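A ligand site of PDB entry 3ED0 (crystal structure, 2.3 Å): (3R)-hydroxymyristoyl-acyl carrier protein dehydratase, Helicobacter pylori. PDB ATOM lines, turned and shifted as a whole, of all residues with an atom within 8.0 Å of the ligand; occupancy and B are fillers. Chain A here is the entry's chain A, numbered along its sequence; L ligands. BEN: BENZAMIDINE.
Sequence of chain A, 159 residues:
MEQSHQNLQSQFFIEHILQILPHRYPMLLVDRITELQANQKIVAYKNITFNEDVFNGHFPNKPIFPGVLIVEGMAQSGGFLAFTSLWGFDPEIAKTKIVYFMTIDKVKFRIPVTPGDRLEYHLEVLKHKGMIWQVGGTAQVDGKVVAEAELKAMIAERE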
ATOM      1  N   GLN A  37       6.066  10.693   1.700  1.00  0.00           N
ATOM      2  CA  GLN A  37       4.920  11.411   2.251  1.00  0.00           C
ATOM      3  C   GLN A  37       3.724  11.223   1.338  1.00  0.00           C
ATOM      4  O   GLN A  37       3.751  11.625   0.201  1.00  0.00           O
ATOM      5  CB  GLN A  37       5.223  12.902   2.343  1.00  0.00           C
ATOM      6  CG  GLN A  37       5.767  13.386   3.658  1.00  0.00           C
ATOM      7  CD  GLN A  37       4.964  12.916   4.847  1.00  0.00           C
ATOM      8  OE1 GLN A  37       3.779  13.207   4.971  1.00  0.00           O
ATOM      9  NE2 GLN A  37       5.624  12.197   5.740  1.00  0.00           N
ATOM     10  N   ALA A  38       2.675  10.611   1.860  1.00  0.00           N
ATOM     11  CA  ALA A  38       1.513  10.296   1.039  1.00  0.00           C
ATOM     12  C   ALA A  38       0.950  11.517   0.314  1.00  0.00           C
ATOM     13  O   ALA A  38       0.783  12.573   0.907  1.00  0.00           O
ATOM     14  CB  ALA A  38       0.451   9.638   1.883  1.00  0.00           C
ATOM     15  N   ASN A  39       0.676  11.353  -0.966  1.00  0.00           N
ATOM     16  CA  ASN A  39       0.054  12.384  -1.789  1.00  0.00           C
ATOM     17  C   ASN A  39       0.941  13.592  -2.072  1.00  0.00           C
ATOM     18  O   ASN A  39       0.498  14.568  -2.647  1.00  0.00           O
ATOM     19  CB  ASN A  39      -1.268  12.837  -1.186  1.00  0.00           C
ATOM     20  CG  ASN A  39      -2.260  11.723  -1.066  1.00  0.00           C
ATOM     21  OD1 ASN A  39      -2.767  11.447   0.005  1.00  0.00           O
ATOM     22  ND2 ASN A  39      -2.525  11.047  -2.166  1.00  0.00           N
ATOM     23  N   GLN A  40       2.200  13.494  -1.670  1.00  0.00           N
ATOM     24  CA  GLN A  40       3.083  14.637  -1.679  1.00  0.00           C
ATOM     25  C   GLN A  40       4.418  14.331  -2.339  1.00  0.00           C
ATOM     26  O   GLN A  40       4.754  14.924  -3.341  1.00  0.00           O
ATOM     27  CB  GLN A  40       3.283  15.202  -0.276  1.00  0.00           C
ATOM     28  CG  GLN A  40       2.158  16.109   0.161  1.00  0.00           C
ATOM     29  CD  GLN A  40       2.455  16.818   1.448  1.00  0.00           C
ATOM     30  OE1 GLN A  40       1.779  16.609   2.443  1.00  0.00           O
ATOM     31  NE2 GLN A  40       3.448  17.674   1.433  1.00  0.00           N
ATOM     32  N   LYS A  41       5.164  13.387  -1.781  1.00  0.00           N
ATOM     33  CA  LYS A  41       6.436  13.060  -2.389  1.00  0.00           C
ATOM     34  C   LYS A  41       7.117  11.784  -1.950  1.00  0.00           C
ATOM     35  O   LYS A  41       6.727  11.136  -0.987  1.00  0.00           O
ATOM     36  CB  LYS A  41       7.419  14.202  -2.194  1.00  0.00           C
ATOM     37  CG  LYS A  41       7.906  14.374  -0.774  1.00  0.00           C
ATOM     38  CD  LYS A  41       9.287  14.986  -0.803  1.00  0.00           C
ATOM     39  CE  LYS A  41       9.791  15.349   0.570  1.00  0.00           C
ATOM     40  NZ  LYS A  41      11.167  15.925   0.422  1.00  0.00           N
ATOM     41  N   ILE A  42       8.180  11.455  -2.687  1.00  0.00           N
ATOM     42  CA  ILE A  42       8.990  10.288  -2.410  1.00  0.00           C
ATOM     43  C   ILE A  42      10.437  10.577  -2.799  1.00  0.00           C
ATOM     44  O   ILE A  42      10.712  11.354  -3.720  1.00  0.00           O
ATOM     45  CB  ILE A  42       8.494   9.043  -3.201  1.00  0.00           C
ATOM     46  CG1 ILE A  42       9.340   7.817  -2.852  1.00  0.00           C
ATOM     47  CG2 ILE A  42       8.536   9.309  -4.687  1.00  0.00           C
ATOM     48  CD1 ILE A  42       8.778   6.508  -3.364  1.00  0.00           C
ATOM     49  N   LEU A 123      10.747  12.771  -6.504  1.00  0.00           N
ATOM     50  CA  LEU A 123       9.503  13.029  -7.200  1.00  0.00           C
ATOM     51  C   LEU A 123       8.489  13.704  -6.290  1.00  0.00           C
ATOM     52  O   LEU A 123       8.364  13.348  -5.121  1.00  0.00           O
ATOM     53  CB  LEU A 123       8.900  11.713  -7.747  1.00  0.00           C
ATOM     54  CG  LEU A 123       9.552  11.042  -8.965  1.00  0.00           C
ATOM     55  CD1 LEU A 123       9.462  11.961 -10.193  1.00  0.00           C
ATOM     56  CD2 LEU A 123      11.013  10.736  -8.648  1.00  0.00           C
ATOM     57  N   GLU A 124       7.780  14.679  -6.841  1.00  0.00           N
ATOM     58  CA  GLU A 124       6.751  15.427  -6.114  1.00  0.00           C
ATOM     59  C   GLU A 124       5.432  15.212  -6.860  1.00  0.00           C
ATOM     60  O   GLU A 124       5.402  15.097  -8.085  1.00  0.00           O
ATOM     61  CB  GLU A 124       7.084  16.922  -6.104  1.00  0.00           C
ATOM     62  CG  GLU A 124       8.549  17.291  -5.795  1.00  0.00           C
ATOM     63  CD  GLU A 124       8.842  17.455  -4.316  1.00  0.00           C
ATOM     64  OE1 GLU A 124       9.513  18.454  -3.952  1.00  0.00           O
ATOM     65  OE2 GLU A 124       8.432  16.609  -3.505  1.00  0.00           O
ATOM     66  N   VAL A 125       4.321  15.180  -6.124  1.00  0.00           N
ATOM     67  CA  VAL A 125       3.006  15.010  -6.723  1.00  0.00           C
ATOM     68  C   VAL A 125       2.469  16.382  -7.149  1.00  0.00           C
ATOM     69  O   VAL A 125       2.188  17.240  -6.317  1.00  0.00           O
ATOM     70  CB  VAL A 125       2.013  14.386  -5.717  1.00  0.00           C
ATOM     71  CG1 VAL A 125       0.615  14.340  -6.312  1.00  0.00           C
ATOM     72  CG2 VAL A 125       2.474  12.984  -5.346  1.00  0.00           C
ATOM     73  N   LEU A 126       2.325  16.584  -8.459  1.00  0.00           N
ATOM     74  CA  LEU A 126       1.845  17.857  -8.977  1.00  0.00           C
ATOM     75  C   LEU A 126       0.329  17.874  -9.046  1.00  0.00           C
ATOM     76  O   LEU A 126      -0.297  18.918  -8.860  1.00  0.00           O
ATOM     77  CB  LEU A 126       2.434  18.129 -10.345  1.00  0.00           C
ATOM     78  CG  LEU A 126       3.962  18.091 -10.416  1.00  0.00           C
ATOM     79  CD1 LEU A 126       4.393  18.174 -11.875  1.00  0.00           C
ATOM     80  CD2 LEU A 126       4.553  19.245  -9.617  1.00  0.00           C
ATOM     81  N   LYS A 127      -0.259  16.714  -9.311  1.00  0.00           N
ATOM     82  CA  LYS A 127      -1.717  16.594  -9.394  1.00  0.00           C
ATOM     83  C   LYS A 127      -2.131  15.124  -9.340  1.00  0.00           C
ATOM     84  O   LYS A 127      -1.490  14.262  -9.937  1.00  0.00           O
ATOM     85  CB  LYS A 127      -2.204  17.220 -10.698  1.00  0.00           C
ATOM     86  CG  LYS A 127      -3.719  17.214 -10.860  1.00  0.00           C
ATOM     87  CD  LYS A 127      -4.112  17.522 -12.304  1.00  0.00           C
ATOM     88  CE  LYS A 127      -5.630  17.653 -12.465  1.00  0.00           C
ATOM     89  NZ  LYS A 127      -6.148  18.885 -11.791  1.00  0.00           N
ATOM     90  N   GLN A 134       0.114  12.790 -11.680  1.00  0.00           N
ATOM     91  CA  GLN A 134       1.113  13.595 -12.390  1.00  0.00           C
ATOM     92  C   GLN A 134       2.216  13.918 -11.412  1.00  0.00           C
ATOM     93  O   GLN A 134       1.978  14.585 -10.399  1.00  0.00           O
ATOM     94  CB  GLN A 134       0.505  14.887 -12.913  1.00  0.00           C
ATOM     95  CG  GLN A 134      -0.333  14.709 -14.164  1.00  0.00           C
ATOM     96  CD  GLN A 134      -1.013  16.000 -14.587  1.00  0.00           C
ATOM     97  OE1 GLN A 134      -0.382  17.058 -14.630  1.00  0.00           O
ATOM     98  NE2 GLN A 134      -2.299  15.911 -14.908  1.00  0.00           N
ATOM     99  N   GLY A 136       6.567  15.024 -10.817  1.00  0.00           N
ATOM    100  CA  GLY A 136       7.662  15.731 -11.433  1.00  0.00           C
ATOM    101  C   GLY A 136       8.782  15.828 -10.428  1.00  0.00           C
ATOM    102  O   GLY A 136       8.538  15.784  -9.216  1.00  0.00           O
HETATM  103  C1  BEN L   1       5.191  19.082  -3.257  1.00  0.00           C
HETATM  104  C2  BEN L   1       6.297  19.816  -3.685  1.00  0.00           C
HETATM  105  C3  BEN L   1       6.280  20.433  -4.934  1.00  0.00           C
HETATM  106  C4  BEN L   1       5.174  20.309  -5.755  1.00  0.00           C
HETATM  107  C5  BEN L   1       4.079  19.571  -5.335  1.00  0.00           C
HETATM  108  C6  BEN L   1       4.082  18.952  -4.090  1.00  0.00           C
HETATM  109  C   BEN L   1       5.208  18.466  -2.008  1.00  0.00           C
HETATM  110  N1  BEN L   1       6.352  18.034  -1.491  1.00  0.00           N
HETATM  111  N2  BEN L   1       4.086  18.347  -1.314  1.00  0.00           N
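Merely in contact with the ligand: Val 125 (3.2 Å).
Of the 13 residues printed, 3 come within 4 Å of the ligand.
NE2 of Gln 40 lies close to N2 of the ligand, 2.9 Å away.
The side-chain carboxylate (OE2) of Glu 124 lies within salt-bridge range of a nitrogen (N1) of the ligand (3.2 Å).
N of Glu 124 sits at hydrogen-bond distance from O of Gly 136 (2.7 Å).
The backbone NH (N) of Val 125 is in hydrogen-bond range of the backbone carbonyl oxygen (O) of Gln 40.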
